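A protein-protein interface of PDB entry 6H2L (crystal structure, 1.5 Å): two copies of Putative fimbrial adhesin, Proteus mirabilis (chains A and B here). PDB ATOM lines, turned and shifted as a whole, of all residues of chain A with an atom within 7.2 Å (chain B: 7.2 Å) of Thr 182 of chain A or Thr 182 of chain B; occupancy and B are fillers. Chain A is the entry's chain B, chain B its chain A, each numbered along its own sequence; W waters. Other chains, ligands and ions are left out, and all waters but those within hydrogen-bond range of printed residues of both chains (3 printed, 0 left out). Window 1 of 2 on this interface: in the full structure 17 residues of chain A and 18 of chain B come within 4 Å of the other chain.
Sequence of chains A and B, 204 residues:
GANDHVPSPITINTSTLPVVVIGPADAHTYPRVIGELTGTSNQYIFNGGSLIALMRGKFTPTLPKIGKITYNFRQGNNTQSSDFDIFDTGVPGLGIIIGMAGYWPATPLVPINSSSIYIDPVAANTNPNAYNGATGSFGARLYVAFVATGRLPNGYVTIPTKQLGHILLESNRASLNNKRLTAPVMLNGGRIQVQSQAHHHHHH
Printed residues of chain B within 4 Å of Thr 182 of chain A: Thr 182 (3.6 Å).
Printed residues of chain A within 4 Å of Thr 182 of chain B: Thr 182.
Of the printed residues of chain A, Lys 179 of chain B touches Gln 163 (3.6 Å) and His 166 (3.4 Å).
Printed residues of chain A within 4 Å of His 166 of chain B: Lys 179 (3.3 Å) and Arg 180 (3.1 Å).
Printed residues of chain A within 4 Å of Leu 181 of chain B: Gln 163 (3.3 Å).
Printed residues of chain B within 4 Å of Gln 163 of chain A: Lys 179 and Leu 181.
The nearest printed residue of chain B that does not touch Thr 182 of chain A is His 166 of chain B (4.1 Å).
O of Lys 179 of chain A lies close to OE1 of Gln 163 of chain B (3.4 Å).
A ring nitrogen (NE2) of His 166 of chain B is in hydrogen-bond range of the backbone carbonyl oxygen (O) of Lys 179 of chain A (3.3 Å).
A ring nitrogen (NE2) of His 166 of chain B lies within hydrogen-bond range of the backbone carbonyl oxygen (O) of Arg 180 of chain A (3.1 Å).
NE2 of His 166 of chain A lies within hydrogen-bond range of O of Lys 179 of chain B (3.4 Å).
O of Arg 180 of chain B is in hydrogen-bond range of NE2 of His 166 of chain A (3.0 Å).
Gln 163 of chain A touches Lys 179 of chain B, and with the chains exchanged Lys 179 of chain A touches Gln 163 of chain B.
Gln 163 of chain A touches Leu 181 of chain B, and with the chains exchanged Leu 181 of chain A touches Gln 163 of chain B.
His 166 of chain A touches Lys 179 of chain B, and with the chains exchanged Lys 179 of chain A touches His 166 of chain B.
His 166 of chain A touches Arg 180 of chain B, and with the chains exchanged Arg 180 of chain A touches His 166 of chain B.
Of the 9 pairs that touch across the chains among the printed residues, 9 have their exchanged pair printed and touching as well.
Among the printed residues, pairs that only touch across the chains: Gln 163 of chain A with Lys 179 of chain B, Gln 163 of chain A with Leu 181 of chain B, Leu 181 of chain A with Gln 163 of chain B and Thr 182 of chain A with Thr 182 of chain B.
Water W2 lies within hydrogen-bond range of the side-chain amide nitrogen (NE2) of Gln 163 of chain B (2.6 Å) and the backbone NH (N) of Thr 182 of chain A (3.1 Å).
Water W3 bridges the side-chain amide nitrogen (NE2) of Gln 163 of chain A and the backbone NH (N) of Thr 182 of chain B.
Water W1 lies within hydrogen-bond range of a ring nitrogen (ND1) of His 166 of chain A, the side-chain hydroxyl (OG1) of Thr 182 of chain A and the side-chain hydroxyl (OG1) of Thr 182 of chain B.
Of the 17 printed residues of chain A, 6 touch a printed residue of chain B.
Printed residues of chain A that touch a printed residue of chain B: Gln 163, His 166, Lys 179, Arg 180, Leu 181 and Thr 182.
Hydrophobic or aromatic side chains of chain A that line the printed part of chain B: His 166 and Leu 181.
Of the 17 printed residues of chain B, 6 touch a printed residue of chain A.
Hydrophobic or aromatic side chains of chain B within 4 Å of the printed part of chain A: His 166 and Leu 181.
Among the printed residues, no Asp or Glu carboxylate lies within 4 Å of a Lys or Arg side-chain nitrogen of the other chain.
NE2 of His 166 of chain B lies within hydrogen-bond range of OE1 of Gln 163 of chain B (2.9 Å).
The backbone carbonyl oxygen (O) of Leu 181 of chain B lies within hydrogen-bond range of the backbone NH (N) of Leu 169 of chain B.
NE2 of His 166 of chain A lies close to OE1 of Gln 163 of chain A, 3.0 Å away.
N of Leu 169 of chain A sits at hydrogen-bond distance from O of Leu 181 of chain A (2.9 Å).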
ATOM      1  N   VAL A   6     -25.510  23.570 -17.790  1.00  0.00           N
ATOM      2  CA  VAL A   6     -24.548  22.984 -16.858  1.00  0.00           C
ATOM      3  C   VAL A   6     -25.058  23.170 -15.432  1.00  0.00           C
ATOM      4  O   VAL A   6     -25.331  24.300 -15.030  1.00  0.00           O
ATOM      5  CB  VAL A   6     -23.163  23.614 -17.026  1.00  0.00           C
ATOM      6  CG1 VAL A   6     -22.224  23.135 -15.911  1.00  0.00           C
ATOM      7  CG2 VAL A   6     -22.607  23.296 -18.377  1.00  0.00           C
ATOM      8  N   PRO A   7     -25.234  22.108 -14.652  1.00  0.00           N
ATOM      9  CA  PRO A   7     -25.664  22.303 -13.261  1.00  0.00           C
ATOM     10  C   PRO A   7     -24.683  23.175 -12.486  1.00  0.00           C
ATOM     11  O   PRO A   7     -23.470  23.030 -12.615  1.00  0.00           O
ATOM     12  CB  PRO A   7     -25.722  20.875 -12.707  1.00  0.00           C
ATOM     13  CG  PRO A   7     -25.949  20.020 -13.908  1.00  0.00           C
ATOM     14  CD  PRO A   7     -25.193  20.674 -15.024  1.00  0.00           C
ATOM     15  N   SER A   8     -25.220  24.039 -11.619  1.00  0.00           N
ATOM     16  CA  SER A   8     -24.420  24.977 -10.840  1.00  0.00           C
ATOM     17  C   SER A   8     -24.200  24.449  -9.429  1.00  0.00           C
ATOM     18  O   SER A   8     -25.129  23.905  -8.832  1.00  0.00           O
ATOM     19  CB  SER A   8     -25.123  26.335 -10.768  1.00  0.00           C
ATOM     20  OG  SER A   8     -24.432  27.240  -9.926  1.00  0.00           O
ATOM     21  N   ILE A  45     -29.812  25.614  -9.162  1.00  0.00           N
ATOM     22  CA  ILE A  45     -28.845  24.523  -9.288  1.00  0.00           C
ATOM     23  C   ILE A  45     -29.033  23.836 -10.634  1.00  0.00           C
ATOM     24  O   ILE A  45     -28.081  23.634 -11.405  1.00  0.00           O
ATOM     25  CB  ILE A  45     -28.986  23.537  -8.115  1.00  0.00           C
ATOM     26  CG1 ILE A  45     -28.598  24.224  -6.801  1.00  0.00           C
ATOM     27  CG2 ILE A  45     -28.110  22.304  -8.362  1.00  0.00           C
ATOM     28  CD1 ILE A  45     -28.823  23.380  -5.554  1.00  0.00           C
ATOM     29  N   PHE A  46     -30.273  23.481 -10.940  1.00  0.00           N
ATOM     30  CA  PHE A  46     -30.653  22.930 -12.230  1.00  0.00           C
ATOM     31  C   PHE A  46     -31.528  23.950 -12.936  1.00  0.00           C
ATOM     32  O   PHE A  46     -32.497  24.453 -12.356  1.00  0.00           O
ATOM     33  CB  PHE A  46     -31.386  21.593 -12.089  1.00  0.00           C
ATOM     34  CG  PHE A  46     -30.582  20.551 -11.360  1.00  0.00           C
ATOM     35  CD1 PHE A  46     -29.543  19.883 -11.996  1.00  0.00           C
ATOM     36  CD2 PHE A  46     -30.854  20.253 -10.025  1.00  0.00           C
ATOM     37  CE1 PHE A  46     -28.810  18.924 -11.318  1.00  0.00           C
ATOM     38  CE2 PHE A  46     -30.092  19.309  -9.338  1.00  0.00           C
ATOM     39  CZ  PHE A  46     -29.082  18.651  -9.991  1.00  0.00           C
ATOM     40  N   LYS A  58     -32.171  14.542  -5.131  1.00  0.00           N
ATOM     41  CA  LYS A  58     -31.672  13.500  -4.246  1.00  0.00           C
ATOM     42  C   LYS A  58     -30.196  13.753  -3.974  1.00  0.00           C
ATOM     43  O   LYS A  58     -29.384  13.806  -4.911  1.00  0.00           O
ATOM     44  CB  LYS A  58     -31.891  12.122  -4.868  1.00  0.00           C
ATOM     45  CG  LYS A  58     -31.645  10.968  -3.909  1.00  0.00           C
ATOM     46  CD  LYS A  58     -31.670   9.623  -4.640  1.00  0.00           C
ATOM     47  CE  LYS A  58     -30.323   9.287  -5.242  1.00  0.00           C
ATOM     48  NZ  LYS A  58     -30.374   8.013  -6.017  1.00  0.00           N
ATOM     49  N   GLN A 163     -15.532  18.478  -1.775  1.00  0.00           N
ATOM     50  CA  GLN A 163     -16.855  18.171  -2.307  1.00  0.00           C
ATOM     51  C   GLN A 163     -17.586  17.308  -1.287  1.00  0.00           C
ATOM     52  O   GLN A 163     -17.086  16.240  -0.904  1.00  0.00           O
ATOM     53  CB  GLN A 163     -16.731  17.442  -3.644  1.00  0.00           C
ATOM     54  CG  GLN A 163     -18.087  17.098  -4.248  1.00  0.00           C
ATOM     55  CD  GLN A 163     -17.980  16.467  -5.614  1.00  0.00           C
ATOM     56  OE1 GLN A 163     -18.316  15.296  -5.801  1.00  0.00           O
ATOM     57  NE2 GLN A 163     -17.491  17.236  -6.580  1.00  0.00           N
ATOM     58  N   HIS A 166     -23.185  15.007  -4.188  1.00  0.00           N
ATOM     59  CA  HIS A 166     -23.866  15.405  -5.411  1.00  0.00           C
ATOM     60  C   HIS A 166     -25.361  15.478  -5.150  1.00  0.00           C
ATOM     61  O   HIS A 166     -25.895  14.730  -4.327  1.00  0.00           O
ATOM     62  CB  HIS A 166     -23.625  14.413  -6.564  1.00  0.00           C
ATOM     63  CG  HIS A 166     -22.188  14.043  -6.761  1.00  0.00           C
ATOM     64  ND1 HIS A 166     -21.378  14.671  -7.683  1.00  0.00           N
ATOM     65  CD2 HIS A 166     -21.421  13.102  -6.165  1.00  0.00           C
ATOM     66  CE1 HIS A 166     -20.174  14.130  -7.645  1.00  0.00           C
ATOM     67  NE2 HIS A 166     -20.170  13.183  -6.726  1.00  0.00           N
ATOM     68  N   ILE A 167     -26.034  16.363  -5.882  1.00  0.00           N
ATOM     69  CA  ILE A 167     -27.494  16.366  -5.971  1.00  0.00           C
ATOM     70  C   ILE A 167     -27.839  15.811  -7.341  1.00  0.00           C
ATOM     71  O   ILE A 167     -27.315  16.291  -8.354  1.00  0.00           O
ATOM     72  CB  ILE A 167     -28.089  17.769  -5.792  1.00  0.00           C
ATOM     73  CG1 ILE A 167     -27.760  18.332  -4.410  1.00  0.00           C
ATOM     74  CG2 ILE A 167     -29.607  17.710  -5.981  1.00  0.00           C
ATOM     75  CD1 ILE A 167     -28.082  19.805  -4.263  1.00  0.00           C
ATOM     76  N   LEU A 168     -28.676  14.784  -7.378  1.00  0.00           N
ATOM     77  CA  LEU A 168     -29.214  14.242  -8.617  1.00  0.00           C
ATOM     78  C   LEU A 168     -30.604  14.826  -8.855  1.00  0.00           C
ATOM     79  O   LEU A 168     -31.450  14.843  -7.949  1.00  0.00           O
ATOM     80  CB  LEU A 168     -29.286  12.723  -8.528  1.00  0.00           C
ATOM     81  CG  LEU A 168     -29.930  11.993  -9.709  1.00  0.00           C
ATOM     82  CD1 LEU A 168     -29.040  12.091 -10.915  1.00  0.00           C
ATOM     83  CD2 LEU A 168     -30.231  10.525  -9.367  1.00  0.00           C
ATOM     84  N   LEU A 169     -30.828  15.330 -10.064  1.00  0.00           N
ATOM     85  CA  LEU A 169     -32.147  15.805 -10.479  1.00  0.00           C
ATOM     86  C   LEU A 169     -32.966  14.634 -11.040  1.00  0.00           C
ATOM     87  O   LEU A 169     -32.544  13.971 -11.992  1.00  0.00           O
ATOM     88  CB  LEU A 169     -32.021  16.895 -11.542  1.00  0.00           C
ATOM     89  CG  LEU A 169     -33.364  17.494 -11.993  1.00  0.00           C
ATOM     90  CD1 LEU A 169     -33.984  18.367 -10.925  1.00  0.00           C
ATOM     91  CD2 LEU A 169     -33.189  18.286 -13.305  1.00  0.00           C
ATOM     92  N   LYS A 179     -31.533  12.125 -18.194  1.00  0.00           N
ATOM     93  CA  LYS A 179     -30.295  12.904 -18.295  1.00  0.00           C
ATOM     94  C   LYS A 179     -29.391  12.685 -17.092  1.00  0.00           C
ATOM     95  O   LYS A 179     -28.175  12.840 -17.205  1.00  0.00           O
ATOM     96  CB  LYS A 179     -30.613  14.401 -18.423  1.00  0.00           C
ATOM     97  CG  LYS A 179     -31.357  14.775 -19.685  1.00  0.00           C
ATOM     98  CD  LYS A 179     -31.389  16.295 -19.838  1.00  0.00           C
ATOM     99  CE  LYS A 179     -32.486  16.739 -20.783  1.00  0.00           C
ATOM    100  NZ  LYS A 179     -32.244  16.223 -22.164  1.00  0.00           N
ATOM    101  N   ARG A 180     -29.962  12.322 -15.943  1.00  0.00           N
ATOM    102  CA  ARG A 180     -29.209  12.150 -14.700  1.00  0.00           C
ATOM    103  C   ARG A 180     -28.301  13.350 -14.437  1.00  0.00           C
ATOM    104  O   ARG A 180     -27.096  13.213 -14.166  1.00  0.00           O
ATOM    105  CB  ARG A 180     -28.423  10.849 -14.717  1.00  0.00           C
ATOM    106  CG  ARG A 180     -29.306   9.609 -14.767  1.00  0.00           C
ATOM    107  CD  ARG A 180     -28.487   8.331 -14.737  1.00  0.00           C
ATOM    108  NE  ARG A 180     -29.337   7.143 -14.796  1.00  0.00           N
ATOM    109  CZ  ARG A 180     -28.878   5.896 -14.880  1.00  0.00           C
ATOM    110  NH1 ARG A 180     -27.571   5.665 -14.921  1.00  0.00           N
ATOM    111  NH2 ARG A 180     -29.730   4.879 -14.932  1.00  0.00           N
ATOM    112  N   LEU A 181     -28.892  14.541 -14.525  1.00  0.00           N
ATOM    113  CA  LEU A 181     -28.171  15.773 -14.215  1.00  0.00           C
ATOM    114  C   LEU A 181     -27.744  15.748 -12.752  1.00  0.00           C
ATOM    115  O   LEU A 181     -28.535  15.426 -11.865  1.00  0.00           O
ATOM    116  CB  LEU A 181     -29.045  16.995 -14.495  1.00  0.00           C
ATOM    117  CG  LEU A 181     -29.576  17.112 -15.921  1.00  0.00           C
ATOM    118  CD1 LEU A 181     -30.398  18.383 -16.052  1.00  0.00           C
ATOM    119  CD2 LEU A 181     -28.455  17.078 -16.942  1.00  0.00           C
ATOM    120  N   THR A 182     -26.490  16.104 -12.499  1.00  0.00           N
ATOM    121  CA  THR A 182     -25.951  16.118 -11.148  1.00  0.00           C
ATOM    122  C   THR A 182     -25.208  17.423 -10.908  1.00  0.00           C
ATOM    123  O   THR A 182     -24.590  17.984 -11.815  1.00  0.00           O
ATOM    124  CB  THR A 182     -25.015  14.934 -10.892  1.00  0.00           C
ATOM    125  OG1 THR A 182     -23.915  14.974 -11.805  1.00  0.00           O
ATOM    126  CG2 THR A 182     -25.763  13.619 -11.054  1.00  0.00           C
ATOM    127  N   ALA A 183     -25.301  17.906  -9.672  1.00  0.00           N
ATOM    128  CA  ALA A 183     -24.640  19.137  -9.265  1.00  0.00           C
ATOM    129  C   ALA A 183     -23.789  18.894  -8.026  1.00  0.00           C
ATOM    130  O   ALA A 183     -24.236  18.203  -7.108  1.00  0.00           O
ATOM    131  CB  ALA A 183     -25.665  20.247  -8.983  1.00  0.00           C
ATOM    132  N   PRO A 184     -22.587  19.471  -7.954  1.00  0.00           N
ATOM    133  CA  PRO A 184     -21.757  19.284  -6.761  1.00  0.00           C
ATOM    134  C   PRO A 184     -22.167  20.181  -5.610  1.00  0.00           C
ATOM    135  O   PRO A 184     -22.579  21.332  -5.787  1.00  0.00           O
ATOM    136  CB  PRO A 184     -20.348  19.621  -7.263  1.00  0.00           C
ATOM    137  CG  PRO A 184     -20.573  20.609  -8.342  1.00  0.00           C
ATOM    138  CD  PRO A 184     -21.888  20.267  -8.986  1.00  0.00           C
ATOM    139  N   VAL B   6     -14.320  22.101  -8.322  1.00  0.00           N
ATOM    140  CA  VAL B   6     -15.531  21.835  -9.096  1.00  0.00           C
ATOM    141  C   VAL B   6     -15.110  21.324 -10.474  1.00  0.00           C
ATOM    142  O   VAL B   6     -14.385  22.032 -11.194  1.00  0.00           O
ATOM    143  CB  VAL B   6     -16.399  23.093  -9.222  1.00  0.00           C
ATOM    144  CG1 VAL B   6     -17.525  22.867 -10.219  1.00  0.00           C
ATOM    145  CG2 VAL B   6     -16.953  23.506  -7.875  1.00  0.00           C
ATOM    146  N   PRO B   7     -15.542  20.131 -10.897  1.00  0.00           N
ATOM    147  CA  PRO B   7     -15.179  19.656 -12.238  1.00  0.00           C
ATOM    148  C   PRO B   7     -15.684  20.605 -13.309  1.00  0.00           C
ATOM    149  O   PRO B   7     -16.792  21.132 -13.217  1.00  0.00           O
ATOM    150  CB  PRO B   7     -15.860  18.284 -12.332  1.00  0.00           C
ATOM    151  CG  PRO B   7     -15.982  17.838 -10.891  1.00  0.00           C
ATOM    152  CD  PRO B   7     -16.241  19.093 -10.114  1.00  0.00           C
ATOM    153  N   SER B   8     -14.853  20.820 -14.324  1.00  0.00           N
ATOM    154  CA  SER B   8     -15.115  21.750 -15.420  1.00  0.00           C
ATOM    155  C   SER B   8     -15.698  21.019 -16.621  1.00  0.00           C
ATOM    156  O   SER B   8     -15.230  19.928 -16.974  1.00  0.00           O
ATOM    157  CB  SER B   8     -13.821  22.453 -15.838  1.00  0.00           C
ATOM    158  OG  SER B   8     -14.041  23.307 -16.952  1.00  0.00           O
ATOM    159  N   ILE B  45     -10.366  19.156 -16.802  1.00  0.00           N
ATOM    160  CA  ILE B  45     -11.720  18.753 -16.429  1.00  0.00           C
ATOM    161  C   ILE B  45     -11.775  18.493 -14.928  1.00  0.00           C
ATOM    162  O   ILE B  45     -12.633  19.025 -14.205  1.00  0.00           O
ATOM    163  CB  ILE B  45     -12.153  17.523 -17.240  1.00  0.00           C
ATOM    164  CG1 ILE B  45     -12.227  17.894 -18.733  1.00  0.00           C
ATOM    165  CG2 ILE B  45     -13.491  17.001 -16.745  1.00  0.00           C
ATOM    166  CD1 ILE B  45     -12.510  16.748 -19.667  1.00  0.00           C
ATOM    167  N   PHE B  46     -10.837  17.685 -14.437  1.00  0.00           N
ATOM    168  CA  PHE B  46     -10.673  17.440 -13.009  1.00  0.00           C
ATOM    169  C   PHE B  46      -9.329  18.005 -12.563  1.00  0.00           C
ATOM    170  O   PHE B  46      -8.309  17.772 -13.214  1.00  0.00           O
ATOM    171  CB  PHE B  46     -10.757  15.949 -12.700  1.00  0.00           C
ATOM    172  CG  PHE B  46     -12.040  15.304 -13.150  1.00  0.00           C
ATOM    173  CD1 PHE B  46     -13.201  15.455 -12.408  1.00  0.00           C
ATOM    174  CD2 PHE B  46     -12.097  14.570 -14.329  1.00  0.00           C
ATOM    175  CE1 PHE B  46     -14.384  14.864 -12.819  1.00  0.00           C
ATOM    176  CE2 PHE B  46     -13.273  13.989 -14.743  1.00  0.00           C
ATOM    177  CZ  PHE B  46     -14.420  14.137 -13.995  1.00  0.00           C
ATOM    178  N   LYS B  58     -14.100   7.700 -17.277  1.00  0.00           N
ATOM    179  CA  LYS B  58     -15.125   6.832 -17.845  1.00  0.00           C
ATOM    180  C   LYS B  58     -16.282   7.705 -18.311  1.00  0.00           C
ATOM    181  O   LYS B  58     -16.882   8.425 -17.503  1.00  0.00           O
ATOM    182  CB  LYS B  58     -15.612   5.818 -16.822  1.00  0.00           C
ATOM    183  CG  LYS B  58     -16.511   4.738 -17.409  1.00  0.00           C
ATOM    184  CD  LYS B  58     -17.203   3.932 -16.303  1.00  0.00           C
ATOM    185  CE  LYS B  58     -18.477   4.633 -15.848  1.00  0.00           C
ATOM    186  NZ  LYS B  58     -19.158   3.946 -14.715  1.00  0.00           N
ATOM    187  N   GLN B 163     -26.736  18.209 -22.931  1.00  0.00           N
ATOM    188  CA  GLN B 163     -25.730  17.428 -22.224  1.00  0.00           C
ATOM    189  C   GLN B 163     -25.583  16.082 -22.912  1.00  0.00           C
ATOM    190  O   GLN B 163     -26.554  15.323 -23.006  1.00  0.00           O
ATOM    191  CB  GLN B 163     -26.120  17.237 -20.768  1.00  0.00           C
ATOM    192  CG  GLN B 163     -25.050  16.532 -19.939  1.00  0.00           C
ATOM    193  CD  GLN B 163     -25.501  16.280 -18.510  1.00  0.00           C
ATOM    194  OE1 GLN B 163     -25.898  15.164 -18.156  1.00  0.00           O
ATOM    195  NE2 GLN B 163     -25.442  17.316 -17.681  1.00  0.00           N
ATOM    196  N   HIS B 166     -21.637  12.294 -19.036  1.00  0.00           N
ATOM    197  CA  HIS B 166     -20.761  12.641 -17.933  1.00  0.00           C
ATOM    198  C   HIS B 166     -19.453  11.873 -18.063  1.00  0.00           C
ATOM    199  O   HIS B 166     -19.413  10.760 -18.600  1.00  0.00           O
ATOM    200  CB  HIS B 166     -21.392  12.305 -16.571  1.00  0.00           C
ATOM    201  CG  HIS B 166     -22.819  12.730 -16.432  1.00  0.00           C
ATOM    202  ND1 HIS B 166     -23.192  13.874 -15.760  1.00  0.00           N
ATOM    203  CD2 HIS B 166     -23.966  12.158 -16.872  1.00  0.00           C
ATOM    204  CE1 HIS B 166     -24.510  13.985 -15.786  1.00  0.00           C
ATOM    205  NE2 HIS B 166     -25.003  12.963 -16.462  1.00  0.00           N
ATOM    206  N   ILE B 167     -18.383  12.464 -17.549  1.00  0.00           N
ATOM    207  CA  ILE B 167     -17.114  11.758 -17.343  1.00  0.00           C
ATOM    208  C   ILE B 167     -16.988  11.521 -15.847  1.00  0.00           C
ATOM    209  O   ILE B 167     -17.139  12.466 -15.054  1.00  0.00           O
ATOM    210  CB  ILE B 167     -15.912  12.557 -17.875  1.00  0.00           C
ATOM    211  CG1 ILE B 167     -16.025  12.792 -19.370  1.00  0.00           C
ATOM    212  CG2 ILE B 167     -14.601  11.820 -17.528  1.00  0.00           C
ATOM    213  CD1 ILE B 167     -15.027  13.801 -19.894  1.00  0.00           C
ATOM    214  N   LEU B 168     -16.763  10.276 -15.457  1.00  0.00           N
ATOM    215  CA  LEU B 168     -16.477   9.910 -14.074  1.00  0.00           C
ATOM    216  C   LEU B 168     -14.974   9.754 -13.883  1.00  0.00           C
ATOM    217  O   LEU B 168     -14.307   9.065 -14.666  1.00  0.00           O
ATOM    218  CB  LEU B 168     -17.189   8.603 -13.709  1.00  0.00           C
ATOM    219  CG  LEU B 168     -16.915   8.034 -12.305  1.00  0.00           C
ATOM    220  CD1 LEU B 168     -17.527   8.885 -11.248  1.00  0.00           C
ATOM    221  CD2 LEU B 168     -17.427   6.598 -12.218  1.00  0.00           C
ATOM    222  N   LEU B 169     -14.449  10.403 -12.852  1.00  0.00           N
ATOM    223  CA  LEU B 169     -13.039  10.264 -12.492  1.00  0.00           C
ATOM    224  C   LEU B 169     -12.866   9.078 -11.551  1.00  0.00           C
ATOM    225  O   LEU B 169     -13.520   9.011 -10.506  1.00  0.00           O
ATOM    226  CB  LEU B 169     -12.514  11.542 -11.835  1.00  0.00           C
ATOM    227  CG  LEU B 169     -11.017  11.543 -11.496  1.00  0.00           C
ATOM    228  CD1 LEU B 169     -10.205  11.608 -12.777  1.00  0.00           C
ATOM    229  CD2 LEU B 169     -10.661  12.674 -10.558  1.00  0.00           C
ATOM    230  N   LYS B 179     -14.696   9.882  -4.133  1.00  0.00           N
ATOM    231  CA  LYS B 179     -15.358  11.162  -4.360  1.00  0.00           C
ATOM    232  C   LYS B 179     -16.358  11.064  -5.506  1.00  0.00           C
ATOM    233  O   LYS B 179     -17.304  11.858  -5.575  1.00  0.00           O
ATOM    234  CB  LYS B 179     -14.336  12.250  -4.693  1.00  0.00           C
ATOM    235  CG  LYS B 179     -13.292  12.507  -3.623  1.00  0.00           C
ATOM    236  CD  LYS B 179     -12.497  13.773  -3.951  1.00  0.00           C
ATOM    237  CE  LYS B 179     -11.125  13.777  -3.291  1.00  0.00           C
ATOM    238  NZ  LYS B 179     -11.181  13.753  -1.798  1.00  0.00           N
ATOM    239  N   ARG B 180     -16.142  10.128  -6.437  1.00  0.00           N
ATOM    240  CA  ARG B 180     -16.994   9.989  -7.621  1.00  0.00           C
ATOM    241  C   ARG B 180     -17.199  11.339  -8.297  1.00  0.00           C
ATOM    242  O   ARG B 180     -18.316  11.737  -8.609  1.00  0.00           O
ATOM    243  CB  ARG B 180     -18.329   9.337  -7.274  1.00  0.00           C
ATOM    244  CG  ARG B 180     -18.196   7.893  -6.808  1.00  0.00           C
ATOM    245  CD  ARG B 180     -19.558   7.266  -6.543  1.00  0.00           C
ATOM    246  NE  ARG B 180     -19.435   5.884  -6.085  1.00  0.00           N
ATOM    247  CZ  ARG B 180     -20.458   5.126  -5.692  1.00  0.00           C
ATOM    248  NH1 ARG B 180     -21.693   5.614  -5.699  1.00  0.00           N
ATOM    249  NH2 ARG B 180     -20.242   3.879  -5.289  1.00  0.00           N
ATOM    250  N   LEU B 181     -16.091  12.038  -8.538  1.00  0.00           N
ATOM    251  CA  LEU B 181     -16.140  13.308  -9.251  1.00  0.00           C
ATOM    252  C   LEU B 181     -16.631  13.082 -10.675  1.00  0.00           C
ATOM    253  O   LEU B 181     -16.189  12.151 -11.361  1.00  0.00           O
ATOM    254  CB  LEU B 181     -14.768  13.965  -9.259  1.00  0.00           C
ATOM    255  CG  LEU B 181     -14.165  14.191  -7.868  1.00  0.00           C
ATOM    256  CD1 LEU B 181     -12.825  14.896  -7.975  1.00  0.00           C
ATOM    257  CD2 LEU B 181     -15.140  14.978  -6.982  1.00  0.00           C
ATOM    258  N   THR B 182     -17.571  13.920 -11.111  1.00  0.00           N
ATOM    259  CA  THR B 182     -18.139  13.813 -12.445  1.00  0.00           C
ATOM    260  C   THR B 182     -18.164  15.179 -13.108  1.00  0.00           C
ATOM    261  O   THR B 182     -18.307  16.212 -12.447  1.00  0.00           O
ATOM    262  CB  THR B 182     -19.563  13.232 -12.406  1.00  0.00           C
ATOM    263  OG1 THR B 182     -20.413  14.082 -11.639  1.00  0.00           O
ATOM    264  CG2 THR B 182     -19.559  11.838 -11.795  1.00  0.00           C
ATOM    265  N   ALA B 183     -18.013  15.172 -14.430  1.00  0.00           N
ATOM    266  CA  ALA B 183     -18.030  16.395 -15.211  1.00  0.00           C
ATOM    267  C   ALA B 183     -18.984  16.259 -16.385  1.00  0.00           C
ATOM    268  O   ALA B 183     -19.060  15.186 -16.974  1.00  0.00           O
ATOM    269  CB  ALA B 183     -16.620  16.730 -15.721  1.00  0.00           C
ATOM    270  N   PRO B 184     -19.742  17.309 -16.715  1.00  0.00           N
ATOM    271  CA  PRO B 184     -20.633  17.227 -17.874  1.00  0.00           C
ATOM    272  C   PRO B 184     -19.915  17.429 -19.202  1.00  0.00           C
ATOM    273  O   PRO B 184     -18.979  18.225 -19.324  1.00  0.00           O
ATOM    274  CB  PRO B 184     -21.645  18.347 -17.618  1.00  0.00           C
ATOM    275  CG  PRO B 184     -20.877  19.372 -16.843  1.00  0.00           C
ATOM    276  CD  PRO B 184     -19.842  18.607 -16.007  1.00  0.00           C
HETATM  277  O   HOH W   1     -22.026  16.537  -9.794  1.00  0.00           O
HETATM  278  O   HOH W   2     -25.026  16.931 -15.105  1.00  0.00           O
HETATM  279  O   HOH W   3     -18.227  16.149  -9.006  1.00  0.00           O
